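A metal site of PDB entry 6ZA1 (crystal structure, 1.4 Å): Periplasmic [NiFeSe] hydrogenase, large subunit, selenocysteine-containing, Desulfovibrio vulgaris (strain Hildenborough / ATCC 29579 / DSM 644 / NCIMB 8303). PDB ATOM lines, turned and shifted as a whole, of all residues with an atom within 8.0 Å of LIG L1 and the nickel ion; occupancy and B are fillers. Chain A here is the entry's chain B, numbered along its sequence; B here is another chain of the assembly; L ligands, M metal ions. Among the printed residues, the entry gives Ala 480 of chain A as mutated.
SE of SEC 478 is bonded to a sulfur (S1) of LIG L1 (2.1 Å).
A sulfur (S1) of LIG L1 lies close to the guanidinium group of Arg 411.
An iron atom (FE1) of LG2 L2 is bound by the side-chain sulfur (SG) of Cys 481.
An iron atom (FE1) of LG2 L2 is bound by the side-chain sulfur of Cys 67.
The backbone NH (N) of Arg 411 sits at hydrogen-bond distance from a nitrogen (N2) of LG2 L2 (3.0 Å).
The guanidinium group (NH1) of Arg 411 sits at hydrogen-bond distance from a nitrogen (N2) of LG2 L2, 3.2 Å away.
N of Ser 434 is in hydrogen-bond range of N1 of LG2 L2.
The side-chain hydroxyl (OG) of Ser 434 lies within hydrogen-bond range of a nitrogen (N1) of LG2 L2 (2.7 Å).
A sulfur (S1) of LG3 L3 sits close to the backbone carbonyl oxygen (O) of Cys 67 (3.6 Å).
A sulfur (S1) of LG3 L3 sits close to the backbone NH (N) of Ala 70 (3.3 Å).
The side-chain amide nitrogen (ND2) of Asn 102 lies close to a sulfur (S1) of LG3 L3, 3.1 Å away.
N of SEC 478 sits at hydrogen-bond distance from the side-chain hydroxyl of Ser 434 (3.0 Å).
A ring nitrogen (NE2) of His 71 sits close to the side-chain sulfur of Cys 481 (3.3 Å).
The side-chain hydroxyl of Ser 432 is in hydrogen-bond range of the backbone carbonyl oxygen of Cys 481 (2.7 Å).
N of Val 66 sits close to SG of Cys 64.
NH1 of Arg 411 sits at hydrogen-bond distance from OG of Ser 106 (2.8 Å).
The guanidinium group (NE) of Arg 411 lies within salt-bridge range of the side-chain carboxylate (OD1) of Asp 476, 2.9 Å away.
The backbone carbonyl oxygen of Val 66 lies within hydrogen-bond range of the side-chain amide nitrogen of Asn 102 (3.0 Å).
Val 66 touches LIG L1.
Five residues have an atom within 4 Å of LIG L1: Cys 64, Val 66, Cys 67, Arg 411 and SEC 478.
Of the 29 residues printed, 4 come within 4 Å of the nickel ion.
The nearest printed residue that does not touch the nickel ion is Arg 411 (4.7 Å).
S1 of LIG L1 is bound to the nickel ion, 2.0 Å away.
The nickel ion is bound by SG of Cys 481 (2.2 Å).
The side-chain sulfur (SG) of Cys 67 is bound to the nickel ion.
The side-chain sulfur (SG) of Cys 64 binds the nickel ion (2.3 Å).
SE of SEC 478 is bound to the nickel ion.
The nickel ion has five donor atoms within binding distance.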
ATOM      1  N   GLU A  17      16.554  -2.324   1.966  1.00  0.00           N
ATOM      2  CA  GLU A  17      17.898  -2.188   2.506  1.00  0.00           C
ATOM      3  C   GLU A  17      18.099  -3.225   3.605  1.00  0.00           C
ATOM      4  O   GLU A  17      17.217  -3.428   4.446  1.00  0.00           O
ATOM      5  CB  GLU A  17      18.179  -0.795   3.072  1.00  0.00           C
ATOM      6  CG  GLU A  17      19.653  -0.552   3.477  1.00  0.00           C
ATOM      7  CD  GLU A  17      20.113  -1.313   4.723  1.00  0.00           C
ATOM      8  OE1 GLU A  17      19.291  -1.556   5.633  1.00  0.00           O
ATOM      9  OE2 GLU A  17      21.316  -1.653   4.779  1.00  0.00           O
ATOM     10  N   GLN A  61      25.825   7.779  11.868  1.00  0.00           N
ATOM     11  CA  GLN A  61      25.386   7.797  10.478  1.00  0.00           C
ATOM     12  C   GLN A  61      25.673   6.475   9.808  1.00  0.00           C
ATOM     13  O   GLN A  61      24.950   6.076   8.886  1.00  0.00           O
ATOM     14  CB  GLN A  61      26.053   8.921   9.713  1.00  0.00           C
ATOM     15  CG  GLN A  61      25.522  10.267  10.098  1.00  0.00           C
ATOM     16  CD  GLN A  61      26.003  11.345   9.167  1.00  0.00           C
ATOM     17  OE1 GLN A  61      25.522  11.462   8.032  1.00  0.00           O
ATOM     18  NE2 GLN A  61      26.953  12.139   9.629  1.00  0.00           N
ATOM     19  N   ILE A  63      25.083   3.708  10.828  1.00  0.00           N
ATOM     20  CA  ILE A  63      23.983   2.753  10.939  1.00  0.00           C
ATOM     21  C   ILE A  63      23.418   2.442   9.564  1.00  0.00           C
ATOM     22  O   ILE A  63      23.047   1.297   9.270  1.00  0.00           O
ATOM     23  CB  ILE A  63      22.900   3.269  11.906  1.00  0.00           C
ATOM     24  CG1 ILE A  63      23.447   3.260  13.341  1.00  0.00           C
ATOM     25  CG2 ILE A  63      21.625   2.446  11.774  1.00  0.00           C
ATOM     26  CD1 ILE A  63      22.601   4.008  14.333  1.00  0.00           C
ATOM     27  N   CYS A  64      23.374   3.449   8.694  1.00  0.00           N
ATOM     28  CA  CYS A  64      22.659   3.318   7.445  1.00  0.00           C
ATOM     29  C   CYS A  64      23.110   4.386   6.466  1.00  0.00           C
ATOM     30  O   CYS A  64      23.103   5.576   6.786  1.00  0.00           O
ATOM     31  CB  CYS A  64      21.157   3.470   7.686  1.00  0.00           C
ATOM     32  SG  CYS A  64      20.217   3.265   6.176  1.00  0.00           S
ATOM     33  N   GLY A  65      23.488   3.954   5.269  1.00  0.00           N
ATOM     34  CA  GLY A  65      23.916   4.874   4.246  1.00  0.00           C
ATOM     35  C   GLY A  65      22.831   5.378   3.328  1.00  0.00           C
ATOM     36  O   GLY A  65      23.107   6.187   2.442  1.00  0.00           O
ATOM     37  N   VAL A  66      21.610   4.891   3.501  1.00  0.00           N
ATOM     38  CA  VAL A  66      20.460   5.423   2.785  1.00  0.00           C
ATOM     39  C   VAL A  66      19.838   6.590   3.549  1.00  0.00           C
ATOM     40  O   VAL A  66      19.457   7.594   2.940  1.00  0.00           O
ATOM     41  CB  VAL A  66      19.424   4.310   2.530  1.00  0.00           C
ATOM     42  CG1 VAL A  66      18.200   4.887   1.816  1.00  0.00           C
ATOM     43  CG2 VAL A  66      20.032   3.165   1.730  1.00  0.00           C
ATOM     44  N   CYS A  67      19.755   6.477   4.881  1.00  0.00           N
ATOM     45  CA  CYS A  67      19.172   7.530   5.703  1.00  0.00           C
ATOM     46  C   CYS A  67      20.137   8.113   6.724  1.00  0.00           C
ATOM     47  O   CYS A  67      19.743   8.401   7.865  1.00  0.00           O
ATOM     48  CB  CYS A  67      17.946   6.978   6.450  1.00  0.00           C
ATOM     49  SG  CYS A  67      18.340   5.717   7.721  1.00  0.00           S
ATOM     50  N   PRO A  68      21.402   8.371   6.359  1.00  0.00           N
ATOM     51  CA  PRO A  68      22.340   8.839   7.379  1.00  0.00           C
ATOM     52  C   PRO A  68      21.985  10.210   7.926  1.00  0.00           C
ATOM     53  O   PRO A  68      22.251  10.478   9.106  1.00  0.00           O
ATOM     54  CB  PRO A  68      23.693   8.830   6.665  1.00  0.00           C
ATOM     55  CG  PRO A  68      23.342   9.015   5.219  1.00  0.00           C
ATOM     56  CD  PRO A  68      22.014   8.304   5.019  1.00  0.00           C
ATOM     57  N   ALA A  70      19.168  11.304   8.757  1.00  0.00           N
ATOM     58  CA  ALA A  70      18.195  11.156   9.835  1.00  0.00           C
ATOM     59  C   ALA A  70      18.901  10.844  11.154  1.00  0.00           C
ATOM     60  O   ALA A  70      18.617  11.453  12.189  1.00  0.00           O
ATOM     61  CB  ALA A  70      17.188  10.061   9.492  1.00  0.00           C
ATOM     62  N   HIS A  71      19.856   9.906  11.124  1.00  0.00           N
ATOM     63  CA  HIS A  71      20.625   9.608  12.323  1.00  0.00           C
ATOM     64  C   HIS A  71      21.492  10.783  12.724  1.00  0.00           C
ATOM     65  O   HIS A  71      21.613  11.092  13.921  1.00  0.00           O
ATOM     66  CB  HIS A  71      21.466   8.357  12.088  1.00  0.00           C
ATOM     67  CG  HIS A  71      20.640   7.114  12.011  1.00  0.00           C
ATOM     68  ND1 HIS A  71      19.991   6.594  13.108  1.00  0.00           N
ATOM     69  CD2 HIS A  71      20.307   6.315  10.967  1.00  0.00           C
ATOM     70  CE1 HIS A  71      19.313   5.520  12.746  1.00  0.00           C
ATOM     71  NE2 HIS A  71      19.487   5.334  11.455  1.00  0.00           N
ATOM     72  N   ASN A 102      17.453  14.904   1.471  1.00  0.00           N
ATOM     73  CA  ASN A 102      17.523  13.451   1.462  1.00  0.00           C
ATOM     74  C   ASN A 102      16.174  12.772   1.555  1.00  0.00           C
ATOM     75  O   ASN A 102      16.055  11.606   1.162  1.00  0.00           O
ATOM     76  CB  ASN A 102      18.424  12.867   2.542  1.00  0.00           C
ATOM     77  CG  ASN A 102      18.908  11.482   2.159  1.00  0.00           C
ATOM     78  OD1 ASN A 102      19.396  11.280   1.044  1.00  0.00           O
ATOM     79  ND2 ASN A 102      18.730  10.517   3.049  1.00  0.00           N
ATOM     80  N   SER A 106      15.479   9.774  -0.892  1.00  0.00           N
ATOM     81  CA  SER A 106      15.124   8.463  -0.362  1.00  0.00           C
ATOM     82  C   SER A 106      13.792   7.975  -0.927  1.00  0.00           C
ATOM     83  O   SER A 106      13.659   6.806  -1.277  1.00  0.00           O
ATOM     84  CB  SER A 106      15.083   8.534   1.160  1.00  0.00           C
ATOM     85  OG  SER A 106      14.853   7.258   1.728  1.00  0.00           O
ATOM     86  N   LEU A 109      14.398   7.089  -4.609  1.00  0.00           N
ATOM     87  CA  LEU A 109      15.097   5.803  -4.634  1.00  0.00           C
ATOM     88  C   LEU A 109      14.140   4.683  -4.312  1.00  0.00           C
ATOM     89  O   LEU A 109      14.142   3.637  -4.988  1.00  0.00           O
ATOM     90  CB  LEU A 109      16.237   5.820  -3.612  1.00  0.00           C
ATOM     91  CG  LEU A 109      16.979   4.500  -3.351  1.00  0.00           C
ATOM     92  CD1 LEU A 109      18.011   4.256  -4.447  1.00  0.00           C
ATOM     93  CD2 LEU A 109      17.634   4.515  -1.979  1.00  0.00           C
ATOM     94  N   LEU A 114      13.738   0.534  -5.810  1.00  0.00           N
ATOM     95  CA  LEU A 114      13.376  -0.611  -4.981  1.00  0.00           C
ATOM     96  C   LEU A 114      12.000  -1.145  -5.337  1.00  0.00           C
ATOM     97  O   LEU A 114      11.850  -2.356  -5.573  1.00  0.00           O
ATOM     98  CB  LEU A 114      13.453  -0.221  -3.483  1.00  0.00           C
ATOM     99  CG  LEU A 114      14.759   0.438  -3.011  1.00  0.00           C
ATOM    100  CD1 LEU A 114      14.726   0.873  -1.550  1.00  0.00           C
ATOM    101  CD2 LEU A 114      15.960  -0.493  -3.229  1.00  0.00           C
ATOM    102  N   ALA A 409      12.765  10.014  10.254  1.00  0.00           N
ATOM    103  CA  ALA A 409      13.557   9.587   9.121  1.00  0.00           C
ATOM    104  C   ALA A 409      12.599   9.363   7.958  1.00  0.00           C
ATOM    105  O   ALA A 409      11.395   9.241   8.162  1.00  0.00           O
ATOM    106  CB  ALA A 409      14.295   8.292   9.448  1.00  0.00           C
ATOM    107  N   PRO A 410      13.105   9.284   6.729  1.00  0.00           N
ATOM    108  CA  PRO A 410      12.193   9.011   5.597  1.00  0.00           C
ATOM    109  C   PRO A 410      11.289   7.805   5.804  1.00  0.00           C
ATOM    110  O   PRO A 410      10.169   7.779   5.268  1.00  0.00           O
ATOM    111  CB  PRO A 410      13.137   8.833   4.406  1.00  0.00           C
ATOM    112  CG  PRO A 410      14.311   9.684   4.752  1.00  0.00           C
ATOM    113  CD  PRO A 410      14.482   9.535   6.269  1.00  0.00           C
ATOM    114  N   ARG A 411      11.731   6.807   6.574  1.00  0.00           N
ATOM    115  CA  ARG A 411      10.948   5.600   6.796  1.00  0.00           C
ATOM    116  C   ARG A 411      10.153   5.622   8.093  1.00  0.00           C
ATOM    117  O   ARG A 411       9.337   4.716   8.303  1.00  0.00           O
ATOM    118  CB  ARG A 411      11.866   4.376   6.757  1.00  0.00           C
ATOM    119  CG  ARG A 411      12.417   4.131   5.382  1.00  0.00           C
ATOM    120  CD  ARG A 411      13.753   3.380   5.289  1.00  0.00           C
ATOM    121  NE  ARG A 411      14.027   3.354   3.860  1.00  0.00           N
ATOM    122  CZ  ARG A 411      14.584   4.366   3.190  1.00  0.00           C
ATOM    123  NH1 ARG A 411      14.983   5.451   3.829  1.00  0.00           N
ATOM    124  NH2 ARG A 411      14.744   4.257   1.880  1.00  0.00           N
ATOM    125  N   SER A 432      14.552   3.266  16.070  1.00  0.00           N
ATOM    126  CA  SER A 432      14.539   3.753  14.699  1.00  0.00           C
ATOM    127  C   SER A 432      13.257   3.362  13.963  1.00  0.00           C
ATOM    128  O   SER A 432      12.419   2.606  14.466  1.00  0.00           O
ATOM    129  CB  SER A 432      15.740   3.170  13.950  1.00  0.00           C
ATOM    130  OG  SER A 432      15.607   1.756  13.930  1.00  0.00           O
ATOM    131  N   ALA A 433      13.128   3.877  12.744  1.00  0.00           N
ATOM    132  CA  ALA A 433      11.886   3.726  11.987  1.00  0.00           C
ATOM    133  C   ALA A 433      11.595   2.269  11.654  1.00  0.00           C
ATOM    134  O   ALA A 433      10.522   1.742  11.986  1.00  0.00           O
ATOM    135  CB  ALA A 433      11.953   4.566  10.710  1.00  0.00           C
ATOM    136  N   SER A 434      12.510   1.601  10.948  1.00  0.00           N
ATOM    137  CA  SER A 434      12.234   0.223  10.554  1.00  0.00           C
ATOM    138  C   SER A 434      12.212  -0.718  11.741  1.00  0.00           C
ATOM    139  O   SER A 434      11.743  -1.858  11.604  1.00  0.00           O
ATOM    140  CB  SER A 434      13.215  -0.244   9.485  1.00  0.00           C
ATOM    141  OG  SER A 434      12.970   0.456   8.287  1.00  0.00           O
ATOM    142  N   ASP A 476       9.095   0.220   2.820  1.00  0.00           N
ATOM    143  CA  ASP A 476      10.432   0.740   2.592  1.00  0.00           C
ATOM    144  C   ASP A 476      11.386   0.318   3.722  1.00  0.00           C
ATOM    145  O   ASP A 476      12.031   1.167   4.338  1.00  0.00           O
ATOM    146  CB  ASP A 476      10.352   2.253   2.483  1.00  0.00           C
ATOM    147  CG  ASP A 476      11.622   2.920   1.974  1.00  0.00           C
ATOM    148  OD1 ASP A 476      12.630   2.281   1.587  1.00  0.00           O
ATOM    149  OD2 ASP A 476      11.573   4.166   1.982  1.00  0.00           O
ATOM    150  N   PRO A 477      11.503  -0.997   3.987  1.00  0.00           N
ATOM    151  CA  PRO A 477      12.306  -1.440   5.118  1.00  0.00           C
ATOM    152  C   PRO A 477      13.772  -1.206   4.967  1.00  0.00           C
ATOM    153  O   PRO A 477      14.326  -1.255   3.873  1.00  0.00           O
ATOM    154  CB  PRO A 477      12.106  -2.966   5.149  1.00  0.00           C
ATOM    155  CG  PRO A 477      10.969  -3.250   4.287  1.00  0.00           C
ATOM    156  CD  PRO A 477      10.878  -2.126   3.285  1.00  0.00           C
ATOM    157  N   SEC A 478      14.454  -0.883   6.065  1.00  0.00           N
ATOM    158  CA  SEC A 478      15.927  -0.869   6.032  1.00  0.00           C
ATOM    159  CB  SEC A 478      16.586   0.413   5.599  1.00  0.00           C
ATOM    160 SE   SEC A 478      16.258   2.045   6.575  1.00  0.00          SE
ATOM    161  C   SEC A 478      16.427  -1.449   7.344  1.00  0.00           C
ATOM    162  O   SEC A 478      16.470  -0.779   8.371  1.00  0.00           O
ATOM    163  N   LEU A 479      16.771  -2.724   7.280  1.00  0.00           N
ATOM    164  CA  LEU A 479      17.138  -3.541   8.441  1.00  0.00           C
ATOM    165  C   LEU A 479      18.421  -3.122   9.118  1.00  0.00           C
ATOM    166  O   LEU A 479      18.618  -3.391  10.292  1.00  0.00           O
ATOM    167  CB  LEU A 479      17.143  -5.022   8.070  1.00  0.00           C
ATOM    168  CG  LEU A 479      15.778  -5.711   8.114  1.00  0.00           C
ATOM    169  CD1 LEU A 479      15.242  -5.812   9.545  1.00  0.00           C
ATOM    170  CD2 LEU A 479      14.752  -4.989   7.242  1.00  0.00           C
ATOM    171  N   ALA A 480      19.294  -2.410   8.397  1.00  0.00           N
ATOM    172  CA  ALA A 480      20.435  -1.796   9.062  1.00  0.00           C
ATOM    173  C   ALA A 480      19.954  -0.828  10.139  1.00  0.00           C
ATOM    174  O   ALA A 480      20.452  -0.852  11.270  1.00  0.00           O
ATOM    175  CB  ALA A 480      21.330  -1.093   8.033  1.00  0.00           C
ATOM    176  N   CYS A 481      18.984   0.021   9.810  1.00  0.00           N
ATOM    177  CA  CYS A 481      18.409   0.908  10.818  1.00  0.00           C
ATOM    178  C   CYS A 481      17.705   0.131  11.920  1.00  0.00           C
ATOM    179  O   CYS A 481      17.794   0.475  13.099  1.00  0.00           O
ATOM    180  CB  CYS A 481      17.394   1.850  10.179  1.00  0.00           C
ATOM    181  SG  CYS A 481      18.150   3.224   9.368  1.00  0.00           S
ATOM    182  N   ALA A 482      16.959  -0.911  11.542  1.00  0.00           N
ATOM    183  CA  ALA A 482      16.127  -1.613  12.517  1.00  0.00           C
ATOM    184  C   ALA A 482      16.965  -2.261  13.605  1.00  0.00           C
ATOM    185  O   ALA A 482      16.561  -2.281  14.773  1.00  0.00           O
ATOM    186  CB  ALA A 482      15.255  -2.645  11.812  1.00  0.00           C
ATOM    187  N   CYS B  18      26.368  -0.797   5.790  1.00  0.00           N
ATOM    188  CA  CYS B  18      25.241   0.113   5.927  1.00  0.00           C
ATOM    189  C   CYS B  18      24.618   0.476   4.582  1.00  0.00           C
ATOM    190  O   CYS B  18      23.716   1.313   4.552  1.00  0.00           O
ATOM    191  CB  CYS B  18      25.675   1.385   6.683  1.00  0.00           C
ATOM    192  SG  CYS B  18      26.479   2.701   5.720  1.00  0.00           S
ATOM    193  N   THR B  19      25.063  -0.155   3.494  1.00  0.00           N
ATOM    194  CA  THR B  19      24.566   0.056   2.120  1.00  0.00           C
ATOM    195  C   THR B  19      25.101   1.390   1.607  1.00  0.00           C
ATOM    196  O   THR B  19      24.790   1.782   0.468  1.00  0.00           O
ATOM    197  CB  THR B  19      23.048  -0.100   2.036  1.00  0.00           C
ATOM    198  OG1 THR B  19      22.704  -1.383   2.590  1.00  0.00           O
ATOM    199  CG2 THR B  19      22.561  -0.062   0.622  1.00  0.00           C
HETATM  200  S1  LIG L   1      17.082   3.647   5.446  1.00  0.00           S
HETATM  201 FE1  LG2 L   2      16.517   4.674   8.523  1.00  0.00          FE
HETATM  202  C1  LG2 L   2      15.217   3.404   8.814  1.00  0.00           C
HETATM  203  N1  LG2 L   2      14.363   2.625   8.963  1.00  0.00           N
HETATM  204  C2  LG2 L   2      15.375   5.677   7.502  1.00  0.00           C
HETATM  205  N2  LG2 L   2      14.648   6.304   6.859  1.00  0.00           N
HETATM  206  C3  LG2 L   2      16.083   5.398  10.124  1.00  0.00           C
HETATM  207  O1  LG2 L   2      15.779   5.823  11.123  1.00  0.00           O
HETATM  208  S1  LG3 L   3      17.643  10.589   5.945  1.00  0.00           S
HETATM  209 NI    NI M   1      18.084   3.465   7.132  1.00  0.00          NI
